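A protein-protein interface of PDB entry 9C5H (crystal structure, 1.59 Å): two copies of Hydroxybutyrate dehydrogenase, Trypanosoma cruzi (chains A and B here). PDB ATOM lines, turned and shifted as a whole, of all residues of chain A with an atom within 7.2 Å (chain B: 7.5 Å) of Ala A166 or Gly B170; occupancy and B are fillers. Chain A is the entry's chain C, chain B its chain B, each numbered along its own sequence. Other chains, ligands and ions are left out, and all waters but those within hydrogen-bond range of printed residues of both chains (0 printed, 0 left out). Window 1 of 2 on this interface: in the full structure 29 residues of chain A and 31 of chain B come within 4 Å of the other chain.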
ATOM      1  N   TRP A 116     -33.503 -19.731 -18.837  1.00  0.00           N
ATOM      2  CA  TRP A 116     -32.582 -20.138 -17.776  1.00  0.00           C
ATOM      3  C   TRP A 116     -31.198 -20.395 -18.365  1.00  0.00           C
ATOM      4  O   TRP A 116     -30.194 -19.821 -17.924  1.00  0.00           O
ATOM      5  CB  TRP A 116     -33.110 -21.393 -17.049  1.00  0.00           C
ATOM      6  CG  TRP A 116     -32.107 -21.958 -16.064  1.00  0.00           C
ATOM      7  CD1 TRP A 116     -31.015 -22.728 -16.359  1.00  0.00           C
ATOM      8  CD2 TRP A 116     -32.096 -21.784 -14.638  1.00  0.00           C
ATOM      9  NE1 TRP A 116     -30.325 -23.033 -15.213  1.00  0.00           N
ATOM     10  CE2 TRP A 116     -30.968 -22.468 -14.141  1.00  0.00           C
ATOM     11  CE3 TRP A 116     -32.930 -21.120 -13.733  1.00  0.00           C
ATOM     12  CZ2 TRP A 116     -30.650 -22.502 -12.783  1.00  0.00           C
ATOM     13  CZ3 TRP A 116     -32.617 -21.158 -12.385  1.00  0.00           C
ATOM     14  CH2 TRP A 116     -31.487 -21.842 -11.923  1.00  0.00           C
ATOM     15  N   ILE A 119     -29.378 -17.214 -19.533  1.00  0.00           N
ATOM     16  CA  ILE A 119     -28.864 -16.402 -18.436  1.00  0.00           C
ATOM     17  C   ILE A 119     -27.615 -17.030 -17.841  1.00  0.00           C
ATOM     18  O   ILE A 119     -26.631 -16.334 -17.561  1.00  0.00           O
ATOM     19  CB  ILE A 119     -29.969 -16.187 -17.383  1.00  0.00           C
ATOM     20  CG1 ILE A 119     -31.005 -15.213 -17.962  1.00  0.00           C
ATOM     21  CG2 ILE A 119     -29.400 -15.658 -16.081  1.00  0.00           C
ATOM     22  CD1 ILE A 119     -32.309 -15.123 -17.206  1.00  0.00           C
ATOM     23  N   ILE A 120     -27.620 -18.348 -17.636  1.00  0.00           N
ATOM     24  CA  ILE A 120     -26.410 -18.996 -17.140  1.00  0.00           C
ATOM     25  C   ILE A 120     -25.277 -18.817 -18.144  1.00  0.00           C
ATOM     26  O   ILE A 120     -24.133 -18.515 -17.773  1.00  0.00           O
ATOM     27  CB  ILE A 120     -26.659 -20.490 -16.849  1.00  0.00           C
ATOM     28  CG1 ILE A 120     -27.759 -20.703 -15.803  1.00  0.00           C
ATOM     29  CG2 ILE A 120     -25.342 -21.157 -16.433  1.00  0.00           C
ATOM     30  CD1 ILE A 120     -27.583 -19.983 -14.501  1.00  0.00           C
ATOM     31  N   LEU A 124     -22.789 -16.104 -16.419  1.00  0.00           N
ATOM     32  CA  LEU A 124     -21.743 -16.868 -15.749  1.00  0.00           C
ATOM     33  C   LEU A 124     -20.732 -17.477 -16.709  1.00  0.00           C
ATOM     34  O   LEU A 124     -19.537 -17.195 -16.604  1.00  0.00           O
ATOM     35  CB  LEU A 124     -22.390 -17.977 -14.907  1.00  0.00           C
ATOM     36  CG  LEU A 124     -21.469 -19.021 -14.274  1.00  0.00           C
ATOM     37  CD1 LEU A 124     -20.394 -18.316 -13.467  1.00  0.00           C
ATOM     38  CD2 LEU A 124     -22.266 -19.988 -13.407  1.00  0.00           C
ATOM     39  N   GLN A 153     -27.863  -9.391  -6.323  1.00  0.00           N
ATOM     40  CA  GLN A 153     -28.508 -10.677  -6.543  1.00  0.00           C
ATOM     41  C   GLN A 153     -27.518 -11.835  -6.566  1.00  0.00           C
ATOM     42  O   GLN A 153     -27.945 -12.986  -6.702  1.00  0.00           O
ATOM     43  CB  GLN A 153     -29.295 -10.656  -7.857  1.00  0.00           C
ATOM     44  CG  GLN A 153     -30.242  -9.470  -8.046  1.00  0.00           C
ATOM     45  CD  GLN A 153     -31.468  -9.507  -7.147  1.00  0.00           C
ATOM     46  OE1 GLN A 153     -31.556 -10.307  -6.216  1.00  0.00           O
ATOM     47  NE2 GLN A 153     -32.426  -8.630  -7.428  1.00  0.00           N
ATOM     48  N   GLY A 154     -26.218 -11.565  -6.482  1.00  0.00           N
ATOM     49  CA  GLY A 154     -25.230 -12.595  -6.259  1.00  0.00           C
ATOM     50  C   GLY A 154     -24.936 -12.874  -4.804  1.00  0.00           C
ATOM     51  O   GLY A 154     -24.178 -13.802  -4.493  1.00  0.00           O
ATOM     52  N   VAL A 156     -27.751 -12.136  -2.262  1.00  0.00           N
ATOM     53  CA  VAL A 156     -29.068 -12.442  -1.719  1.00  0.00           C
ATOM     54  C   VAL A 156     -29.972 -12.839  -2.875  1.00  0.00           C
ATOM     55  O   VAL A 156     -29.677 -12.589  -4.044  1.00  0.00           O
ATOM     56  CB  VAL A 156     -29.696 -11.257  -0.953  1.00  0.00           C
ATOM     57  CG1 VAL A 156     -28.880 -10.951   0.282  1.00  0.00           C
ATOM     58  CG2 VAL A 156     -29.827 -10.015  -1.836  1.00  0.00           C
ATOM     59  N   LYS A 161     -36.481 -14.191  -9.853  1.00  0.00           N
ATOM     60  CA  LYS A 161     -35.187 -13.988 -10.483  1.00  0.00           C
ATOM     61  C   LYS A 161     -34.273 -15.179 -10.244  1.00  0.00           C
ATOM     62  O   LYS A 161     -33.066 -15.027 -10.049  1.00  0.00           O
ATOM     63  CB  LYS A 161     -34.562 -12.688  -9.982  1.00  0.00           C
ATOM     64  CG  LYS A 161     -35.328 -11.461 -10.467  1.00  0.00           C
ATOM     65  CD  LYS A 161     -34.729 -10.134 -10.006  1.00  0.00           C
ATOM     66  CE  LYS A 161     -35.489  -8.959 -10.635  1.00  0.00           C
ATOM     67  NZ  LYS A 161     -34.986  -7.623 -10.204  1.00  0.00           N
ATOM     68  N   SER A 162     -34.827 -16.394 -10.330  1.00  0.00           N
ATOM     69  CA  SER A 162     -34.068 -17.586  -9.958  1.00  0.00           C
ATOM     70  C   SER A 162     -32.821 -17.760 -10.825  1.00  0.00           C
ATOM     71  O   SER A 162     -31.721 -17.983 -10.306  1.00  0.00           O
ATOM     72  CB  SER A 162     -34.964 -18.827 -10.040  1.00  0.00           C
ATOM     73  OG  SER A 162     -35.546 -18.998 -11.322  1.00  0.00           O
ATOM     74  N   ALA A 163     -32.967 -17.680 -12.150  1.00  0.00           N
ATOM     75  CA  ALA A 163     -31.809 -17.904 -13.014  1.00  0.00           C
ATOM     76  C   ALA A 163     -30.750 -16.829 -12.801  1.00  0.00           C
ATOM     77  O   ALA A 163     -29.551 -17.122 -12.746  1.00  0.00           O
ATOM     78  CB  ALA A 163     -32.226 -17.937 -14.484  1.00  0.00           C
ATOM     79  N   TYR A 164     -31.176 -15.577 -12.693  1.00  0.00           N
ATOM     80  CA  TYR A 164     -30.231 -14.472 -12.554  1.00  0.00           C
ATOM     81  C   TYR A 164     -29.498 -14.528 -11.223  1.00  0.00           C
ATOM     82  O   TYR A 164     -28.274 -14.356 -11.178  1.00  0.00           O
ATOM     83  CB  TYR A 164     -31.010 -13.176 -12.719  1.00  0.00           C
ATOM     84  CG  TYR A 164     -30.264 -11.877 -12.698  1.00  0.00           C
ATOM     85  CD1 TYR A 164     -30.046 -11.204 -11.509  1.00  0.00           C
ATOM     86  CD2 TYR A 164     -29.861 -11.275 -13.878  1.00  0.00           C
ATOM     87  CE1 TYR A 164     -29.407  -9.982 -11.491  1.00  0.00           C
ATOM     88  CE2 TYR A 164     -29.219 -10.056 -13.872  1.00  0.00           C
ATOM     89  CZ  TYR A 164     -29.001  -9.410 -12.679  1.00  0.00           C
ATOM     90  OH  TYR A 164     -28.368  -8.189 -12.680  1.00  0.00           O
ATOM     91  N   CYS A 165     -30.222 -14.778 -10.130  1.00  0.00           N
ATOM     92  CA  CYS A 165     -29.565 -14.922  -8.836  1.00  0.00           C
ATOM     93  C   CYS A 165     -28.610 -16.108  -8.835  1.00  0.00           C
ATOM     94  O   CYS A 165     -27.518 -16.037  -8.263  1.00  0.00           O
ATOM     95  CB  CYS A 165     -30.609 -15.074  -7.731  1.00  0.00           C
ATOM     96  SG  CYS A 165     -31.537 -13.565  -7.385  1.00  0.00           S
ATOM     97  N   ALA A 166     -29.000 -17.214  -9.473  1.00  0.00           N
ATOM     98  CA  ALA A 166     -28.093 -18.351  -9.570  1.00  0.00           C
ATOM     99  C   ALA A 166     -26.826 -17.976 -10.337  1.00  0.00           C
ATOM    100  O   ALA A 166     -25.710 -18.276  -9.900  1.00  0.00           O
ATOM    101  CB  ALA A 166     -28.802 -19.532 -10.232  1.00  0.00           C
ATOM    102  N   ALA A 167     -26.980 -17.310 -11.482  1.00  0.00           N
ATOM    103  CA  ALA A 167     -25.816 -16.966 -12.294  1.00  0.00           C
ATOM    104  C   ALA A 167     -24.906 -15.980 -11.571  1.00  0.00           C
ATOM    105  O   ALA A 167     -23.675 -16.085 -11.645  1.00  0.00           O
ATOM    106  CB  ALA A 167     -26.265 -16.386 -13.634  1.00  0.00           C
ATOM    107  N   LYS A 168     -25.497 -15.002 -10.890  1.00  0.00           N
ATOM    108  CA  LYS A 168     -24.699 -13.975 -10.224  1.00  0.00           C
ATOM    109  C   LYS A 168     -24.017 -14.519  -8.971  1.00  0.00           C
ATOM    110  O   LYS A 168     -22.870 -14.149  -8.681  1.00  0.00           O
ATOM    111  CB  LYS A 168     -25.584 -12.777  -9.887  1.00  0.00           C
ATOM    112  CG  LYS A 168     -26.100 -11.999 -11.097  1.00  0.00           C
ATOM    113  CD  LYS A 168     -24.972 -11.364 -11.901  1.00  0.00           C
ATOM    114  CE  LYS A 168     -25.507 -10.346 -12.905  1.00  0.00           C
ATOM    115  NZ  LYS A 168     -24.419  -9.753 -13.740  1.00  0.00           N
ATOM    116  N   HIS A 169     -24.706 -15.372  -8.200  1.00  0.00           N
ATOM    117  CA  HIS A 169     -24.040 -16.112  -7.126  1.00  0.00           C
ATOM    118  C   HIS A 169     -22.871 -16.913  -7.700  1.00  0.00           C
ATOM    119  O   HIS A 169     -21.743 -16.861  -7.192  1.00  0.00           O
ATOM    120  CB  HIS A 169     -25.037 -17.048  -6.406  1.00  0.00           C
ATOM    121  CG  HIS A 169     -25.825 -16.408  -5.290  1.00  0.00           C
ATOM    122  ND1 HIS A 169     -26.818 -15.480  -5.516  1.00  0.00           N
ATOM    123  CD2 HIS A 169     -25.800 -16.605  -3.949  1.00  0.00           C
ATOM    124  CE1 HIS A 169     -27.351 -15.112  -4.364  1.00  0.00           C
ATOM    125  NE2 HIS A 169     -26.752 -15.780  -3.395  1.00  0.00           N
ATOM    126  N   GLY A 170     -23.117 -17.630  -8.799  1.00  0.00           N
ATOM    127  CA  GLY A 170     -22.054 -18.399  -9.429  1.00  0.00           C
ATOM    128  C   GLY A 170     -20.877 -17.547  -9.873  1.00  0.00           C
ATOM    129  O   GLY A 170     -19.722 -17.962  -9.755  1.00  0.00           O
ATOM    130  N   LEU A 171     -21.156 -16.357 -10.411  1.00  0.00           N
ATOM    131  CA  LEU A 171     -20.084 -15.467 -10.852  1.00  0.00           C
ATOM    132  C   LEU A 171     -19.215 -15.040  -9.679  1.00  0.00           C
ATOM    133  O   LEU A 171     -17.990 -14.919  -9.813  1.00  0.00           O
ATOM    134  CB  LEU A 171     -20.681 -14.249 -11.546  1.00  0.00           C
ATOM    135  CG  LEU A 171     -19.690 -13.275 -12.183  1.00  0.00           C
ATOM    136  CD1 LEU A 171     -18.851 -13.922 -13.255  1.00  0.00           C
ATOM    137  CD2 LEU A 171     -20.498 -12.112 -12.739  1.00  0.00           C
ATOM    138  N   ILE A 172     -19.827 -14.815  -8.521  1.00  0.00           N
ATOM    139  CA  ILE A 172     -19.059 -14.469  -7.333  1.00  0.00           C
ATOM    140  C   ILE A 172     -18.218 -15.658  -6.876  1.00  0.00           C
ATOM    141  O   ILE A 172     -17.049 -15.497  -6.504  1.00  0.00           O
ATOM    142  CB  ILE A 172     -20.011 -13.944  -6.236  1.00  0.00           C
ATOM    143  CG1 ILE A 172     -20.541 -12.569  -6.675  1.00  0.00           C
ATOM    144  CG2 ILE A 172     -19.321 -13.907  -4.895  1.00  0.00           C
ATOM    145  CD1 ILE A 172     -21.579 -11.967  -5.752  1.00  0.00           C
ATOM    146  N   GLY A 173     -18.775 -16.868  -6.926  1.00  0.00           N
ATOM    147  CA  GLY A 173     -17.979 -18.037  -6.583  1.00  0.00           C
ATOM    148  C   GLY A 173     -16.796 -18.211  -7.514  1.00  0.00           C
ATOM    149  O   GLY A 173     -15.680 -18.506  -7.074  1.00  0.00           O
ATOM    150  N   ASN B 123     -24.791 -29.901 -11.420  1.00  0.00           N
ATOM    151  CA  ASN B 123     -24.726 -29.402 -10.055  1.00  0.00           C
ATOM    152  C   ASN B 123     -25.619 -28.190  -9.819  1.00  0.00           C
ATOM    153  O   ASN B 123     -25.863 -27.847  -8.655  1.00  0.00           O
ATOM    154  CB  ASN B 123     -23.280 -29.045  -9.690  1.00  0.00           C
ATOM    155  CG  ASN B 123     -22.365 -30.260  -9.648  1.00  0.00           C
ATOM    156  OD1 ASN B 123     -22.710 -31.329 -10.148  1.00  0.00           O
ATOM    157  ND2 ASN B 123     -21.190 -30.095  -9.051  1.00  0.00           N
ATOM    158  N   LEU B 124     -26.049 -27.497 -10.879  1.00  0.00           N
ATOM    159  CA  LEU B 124     -26.968 -26.371 -10.746  1.00  0.00           C
ATOM    160  C   LEU B 124     -28.251 -26.541 -11.551  1.00  0.00           C
ATOM    161  O   LEU B 124     -29.336 -26.605 -10.967  1.00  0.00           O
ATOM    162  CB  LEU B 124     -26.243 -25.084 -11.168  1.00  0.00           C
ATOM    163  CG  LEU B 124     -27.085 -23.815 -11.279  1.00  0.00           C
ATOM    164  CD1 LEU B 124     -27.807 -23.585  -9.949  1.00  0.00           C
ATOM    165  CD2 LEU B 124     -26.263 -22.599 -11.642  1.00  0.00           C
ATOM    166  N   PHE B 128     -32.695 -27.032 -10.718  1.00  0.00           N
ATOM    167  CA  PHE B 128     -33.760 -26.162 -11.212  1.00  0.00           C
ATOM    168  C   PHE B 128     -34.833 -26.955 -11.946  1.00  0.00           C
ATOM    169  O   PHE B 128     -36.031 -26.764 -11.715  1.00  0.00           O
ATOM    170  CB  PHE B 128     -33.156 -25.093 -12.126  1.00  0.00           C
ATOM    171  CG  PHE B 128     -34.129 -24.473 -13.093  1.00  0.00           C
ATOM    172  CD1 PHE B 128     -35.223 -23.755 -12.638  1.00  0.00           C
ATOM    173  CD2 PHE B 128     -33.924 -24.573 -14.462  1.00  0.00           C
ATOM    174  CE1 PHE B 128     -36.106 -23.173 -13.526  1.00  0.00           C
ATOM    175  CE2 PHE B 128     -34.801 -23.984 -15.355  1.00  0.00           C
ATOM    176  CZ  PHE B 128     -35.893 -23.285 -14.886  1.00  0.00           C
ATOM    177  N   GLN B 153     -18.043 -25.182  -0.744  1.00  0.00           N
ATOM    178  CA  GLN B 153     -17.606 -24.552  -1.982  1.00  0.00           C
ATOM    179  C   GLN B 153     -18.690 -23.682  -2.600  1.00  0.00           C
ATOM    180  O   GLN B 153     -18.435 -23.038  -3.622  1.00  0.00           O
ATOM    181  CB  GLN B 153     -17.163 -25.606  -3.004  1.00  0.00           C
ATOM    182  CG  GLN B 153     -16.192 -26.659  -2.490  1.00  0.00           C
ATOM    183  CD  GLN B 153     -14.795 -26.129  -2.223  1.00  0.00           C
ATOM    184  OE1 GLN B 153     -14.549 -24.922  -2.243  1.00  0.00           O
ATOM    185  NE2 GLN B 153     -13.869 -27.042  -1.958  1.00  0.00           N
ATOM    186  N   GLY B 154     -19.900 -23.681  -2.031  1.00  0.00           N
ATOM    187  CA  GLY B 154     -20.923 -22.726  -2.403  1.00  0.00           C
ATOM    188  C   GLY B 154     -20.892 -21.436  -1.625  1.00  0.00           C
ATOM    189  O   GLY B 154     -21.635 -20.503  -1.947  1.00  0.00           O
ATOM    190  N   TYR B 164     -17.046 -26.002 -10.121  1.00  0.00           N
ATOM    191  CA  TYR B 164     -17.793 -26.550  -8.994  1.00  0.00           C
ATOM    192  C   TYR B 164     -18.178 -25.460  -8.010  1.00  0.00           C
ATOM    193  O   TYR B 164     -19.333 -25.401  -7.567  1.00  0.00           O
ATOM    194  CB  TYR B 164     -16.936 -27.631  -8.338  1.00  0.00           C
ATOM    195  CG  TYR B 164     -17.516 -28.432  -7.195  1.00  0.00           C
ATOM    196  CD1 TYR B 164     -17.410 -27.981  -5.888  1.00  0.00           C
ATOM    197  CD2 TYR B 164     -18.102 -29.674  -7.416  1.00  0.00           C
ATOM    198  CE1 TYR B 164     -17.902 -28.722  -4.834  1.00  0.00           C
ATOM    199  CE2 TYR B 164     -18.599 -30.425  -6.366  1.00  0.00           C
ATOM    200  CZ  TYR B 164     -18.486 -29.950  -5.077  1.00  0.00           C
ATOM    201  OH  TYR B 164     -18.970 -30.695  -4.031  1.00  0.00           O
ATOM    202  N   CYS B 165     -17.240 -24.575  -7.664  1.00  0.00           N
ATOM    203  CA  CYS B 165     -17.578 -23.477  -6.769  1.00  0.00           C
ATOM    204  C   CYS B 165     -18.640 -22.589  -7.393  1.00  0.00           C
ATOM    205  O   CYS B 165     -19.552 -22.115  -6.704  1.00  0.00           O
ATOM    206  CB  CYS B 165     -16.335 -22.659  -6.426  1.00  0.00           C
ATOM    207  SG  CYS B 165     -15.177 -23.510  -5.335  1.00  0.00           S
ATOM    208  N   ALA B 166     -18.535 -22.345  -8.702  1.00  0.00           N
ATOM    209  CA  ALA B 166     -19.530 -21.521  -9.376  1.00  0.00           C
ATOM    210  C   ALA B 166     -20.903 -22.175  -9.308  1.00  0.00           C
ATOM    211  O   ALA B 166     -21.892 -21.535  -8.941  1.00  0.00           O
ATOM    212  CB  ALA B 166     -19.120 -21.277 -10.827  1.00  0.00           C
ATOM    213  N   ALA B 167     -20.974 -23.470  -9.637  1.00  0.00           N
ATOM    214  CA  ALA B 167     -22.254 -24.169  -9.632  1.00  0.00           C
ATOM    215  C   ALA B 167     -22.863 -24.220  -8.235  1.00  0.00           C
ATOM    216  O   ALA B 167     -24.079 -24.060  -8.075  1.00  0.00           O
ATOM    217  CB  ALA B 167     -22.078 -25.587 -10.181  1.00  0.00           C
ATOM    218  N   LYS B 168     -22.035 -24.469  -7.216  1.00  0.00           N
ATOM    219  CA  LYS B 168     -22.543 -24.600  -5.854  1.00  0.00           C
ATOM    220  C   LYS B 168     -22.963 -23.248  -5.288  1.00  0.00           C
ATOM    221  O   LYS B 168     -23.974 -23.157  -4.579  1.00  0.00           O
ATOM    222  CB  LYS B 168     -21.490 -25.259  -4.964  1.00  0.00           C
ATOM    223  CG  LYS B 168     -21.208 -26.724  -5.309  1.00  0.00           C
ATOM    224  CD  LYS B 168     -22.421 -27.622  -5.089  1.00  0.00           C
ATOM    225  CE  LYS B 168     -22.036 -29.095  -5.200  1.00  0.00           C
ATOM    226  NZ  LYS B 168     -23.199 -29.980  -4.906  1.00  0.00           N
ATOM    227  N   HIS B 169     -22.199 -22.191  -5.582  1.00  0.00           N
ATOM    228  CA  HIS B 169     -22.651 -20.842  -5.245  1.00  0.00           C
ATOM    229  C   HIS B 169     -23.994 -20.570  -5.910  1.00  0.00           C
ATOM    230  O   HIS B 169     -24.939 -20.083  -5.278  1.00  0.00           O
ATOM    231  CB  HIS B 169     -21.630 -19.787  -5.700  1.00  0.00           C
ATOM    232  CG  HIS B 169     -20.539 -19.487  -4.712  1.00  0.00           C
ATOM    233  ND1 HIS B 169     -19.536 -20.385  -4.413  1.00  0.00           N
ATOM    234  CD2 HIS B 169     -20.255 -18.362  -4.010  1.00  0.00           C
ATOM    235  CE1 HIS B 169     -18.702 -19.839  -3.545  1.00  0.00           C
ATOM    236  NE2 HIS B 169     -19.114 -18.612  -3.287  1.00  0.00           N
ATOM    237  N   GLY B 170     -24.095 -20.904  -7.200  1.00  0.00           N
ATOM    238  CA  GLY B 170     -25.345 -20.717  -7.916  1.00  0.00           C
ATOM    239  C   GLY B 170     -26.497 -21.492  -7.308  1.00  0.00           C
ATOM    240  O   GLY B 170     -27.622 -20.994  -7.242  1.00  0.00           O
ATOM    241  N   LEU B 171     -26.233 -22.723  -6.856  1.00  0.00           N
ATOM    242  CA  LEU B 171     -27.273 -23.536  -6.231  1.00  0.00           C
ATOM    243  C   LEU B 171     -27.789 -22.888  -4.952  1.00  0.00           C
ATOM    244  O   LEU B 171     -28.988 -22.958  -4.647  1.00  0.00           O
ATOM    245  CB  LEU B 171     -26.726 -24.936  -5.946  1.00  0.00           C
ATOM    246  CG  LEU B 171     -27.707 -25.962  -5.379  1.00  0.00           C
ATOM    247  CD1 LEU B 171     -28.846 -26.222  -6.347  1.00  0.00           C
ATOM    248  CD2 LEU B 171     -26.971 -27.259  -5.036  1.00  0.00           C
ATOM    249  N   ILE B 172     -26.897 -22.254  -4.190  1.00  0.00           N
ATOM    250  CA  ILE B 172     -27.315 -21.532  -2.991  1.00  0.00           C
ATOM    251  C   ILE B 172     -28.148 -20.311  -3.359  1.00  0.00           C
ATOM    252  O   ILE B 172     -29.179 -20.045  -2.734  1.00  0.00           O
ATOM    253  CB  ILE B 172     -26.081 -21.181  -2.136  1.00  0.00           C
ATOM    254  CG1 ILE B 172     -25.532 -22.480  -1.540  1.00  0.00           C
ATOM    255  CG2 ILE B 172     -26.431 -20.170  -1.058  1.00  0.00           C
ATOM    256  CD1 ILE B 172     -24.211 -22.337  -0.853  1.00  0.00           C
ATOM    257  N   GLY B 173     -27.745 -19.569  -4.392  1.00  0.00           N
ATOM    258  CA  GLY B 173     -28.576 -18.463  -4.848  1.00  0.00           C
ATOM    259  C   GLY B 173     -29.954 -18.919  -5.294  1.00  0.00           C
ATOM    260  O   GLY B 173     -30.967 -18.287  -4.973  1.00  0.00           O
ATOM    261  N   PHE B 174     -30.010 -20.032  -6.028  1.00  0.00           N
ATOM    262  CA  PHE B 174     -31.284 -20.597  -6.454  1.00  0.00           C
ATOM    263  C   PHE B 174     -32.149 -20.960  -5.253  1.00  0.00           C
ATOM    264  O   PHE B 174     -33.359 -20.701  -5.246  1.00  0.00           O
ATOM    265  CB  PHE B 174     -31.023 -21.828  -7.325  1.00  0.00           C
ATOM    266  CG  PHE B 174     -32.270 -22.534  -7.767  1.00  0.00           C
ATOM    267  CD1 PHE B 174     -33.122 -21.945  -8.681  1.00  0.00           C
ATOM    268  CD2 PHE B 174     -32.594 -23.781  -7.262  1.00  0.00           C
ATOM    269  CE1 PHE B 174     -34.284 -22.587  -9.088  1.00  0.00           C
ATOM    270  CE2 PHE B 174     -33.753 -24.429  -7.669  1.00  0.00           C
ATOM    271  CZ  PHE B 174     -34.594 -23.830  -8.586  1.00  0.00           C
ATOM    272  N   THR B 175     -31.534 -21.561  -4.232  1.00  0.00           N
ATOM    273  CA  THR B 175     -32.242 -21.944  -3.014  1.00  0.00           C
ATOM    274  C   THR B 175     -32.939 -20.749  -2.397  1.00  0.00           C
ATOM    275  O   THR B 175     -34.107 -20.828  -1.991  1.00  0.00           O
ATOM    276  CB  THR B 175     -31.234 -22.537  -2.027  1.00  0.00           C
ATOM    277  OG1 THR B 175     -30.654 -23.718  -2.596  1.00  0.00           O
ATOM    278  CG2 THR B 175     -31.848 -22.896  -0.691  1.00  0.00           C
ATOM    279  N   LYS B 176     -32.230 -19.627  -2.319  1.00  0.00           N
ATOM    280  CA  LYS B 176     -32.806 -18.425  -1.741  1.00  0.00           C
ATOM    281  C   LYS B 176     -34.060 -18.009  -2.494  1.00  0.00           C
ATOM    282  O   LYS B 176     -35.094 -17.723  -1.883  1.00  0.00           O
ATOM    283  CB  LYS B 176     -31.775 -17.300  -1.752  1.00  0.00           C
ATOM    284  CG  LYS B 176     -30.605 -17.562  -0.845  1.00  0.00           C
ATOM    285  CD  LYS B 176     -29.599 -16.440  -0.905  1.00  0.00           C
ATOM    286  CE  LYS B 176     -28.283 -16.926  -0.327  1.00  0.00           C
ATOM    287  NZ  LYS B 176     -27.167 -15.971  -0.536  1.00  0.00           N
ATOM    288  N   VAL B 177     -33.991 -17.979  -3.827  1.00  0.00           N
ATOM    289  CA  VAL B 177     -35.126 -17.489  -4.605  1.00  0.00           C
ATOM    290  C   VAL B 177     -36.330 -18.405  -4.428  1.00  0.00           C
ATOM    291  O   VAL B 177     -37.455 -17.937  -4.214  1.00  0.00           O
ATOM    292  CB  VAL B 177     -34.749 -17.346  -6.091  1.00  0.00           C
ATOM    293  CG1 VAL B 177     -35.971 -16.956  -6.920  1.00  0.00           C
ATOM    294  CG2 VAL B 177     -33.652 -16.307  -6.274  1.00  0.00           C
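The backbone carbonyl oxygen (O) of Gly A154 lies close to a ring nitrogen (ND1) of His A169.
The backbone carbonyl oxygen (O) of Lys A161 sits close to the side-chain sulfur (SG) of Cys A165.
O of Gln A153 lies within hydrogen-bond range of ND1 of His A169 (3.0 Å).
ND1 of His A169 is in hydrogen-bond range of O of Cys A165, 2.9 Å away.
ND1 of His B169 is in hydrogen-bond range of O of Cys B165 (2.9 Å).
O of Gln B153 sits at hydrogen-bond distance from ND1 of His B169 (3.0 Å).
Among the printed residues, merely in contact across the chains: Ala A166 with Gly B170 (3.2 Å), Gly A170 with Ala B166 (3.2 Å), His A169 with His B169 (3.2 Å), Trp A116 with Phe B128 (3.3 Å), Gly A173 with His B169 (3.5 Å), His A169 with Gly B173 (3.5 Å), Cys A165 with Val B177 (3.6 Å), Trp A116 with Phe B174 (3.6 Å), Ser A162 with Val B177 (3.6 Å), Gly A170 with Gly B170 (3.8 Å), Ser A162 with Phe B174 (3.9 Å) and His A169 with Gly B170 (3.98 Å).
His B169 touches its own counterpart, His A169.
His A169 touches Gly B170, but with the chains exchanged Gly A170 does not touch His B169 (4.001 Å).
His A169 touches Gly B173, and with the chains exchanged Gly A173 touches His B169.
Gly B170 touches its own counterpart, Gly A170.
13 positions are printed for both chains.
Of the 13 pairs that touch across the chains among the printed residues, 6 have their exchanged pair printed and touching as well.
Of the 20 printed residues of chain A, 7 touch a printed residue of chain B.
Hydrophobic or aromatic side chains of chain A within 4 Å of the printed part of chain B: Trp A116, Ala A166 and His A169.
Of the 19 printed residues of chain B, 8 touch a printed residue of chain A.
Among the printed residues, 13 pairs touch across the chains.
Among the printed residues, no Asp or Glu carboxylate lies within 4 Å of a Lys or Arg side-chain nitrogen of the other chain.
Of chain B, only Gly B170 (3.2 Å) comes within 4 Å of Ala A166.
Of chain A, only Ala A166, His A169 and Gly A170 come within 4 Å of Gly B170.
Of the printed residues of chain A, Lys B176 touches His A169 (2.9 Å).
Printed residues of chain B within 4 Å of Trp A116: Phe B128 (3.3 Å) and Phe B174 (3.6 Å).
Gln A153 touches none of the printed residues of chain B.
Lys A161 touches none of the printed residues of chain B.
The nearest residue of chain B that does not touch Ala A166 is Leu B124 (4.2 Å).
NZ of Lys B176 lies within hydrogen-bond range of NE2 of His A169 (2.9 Å).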
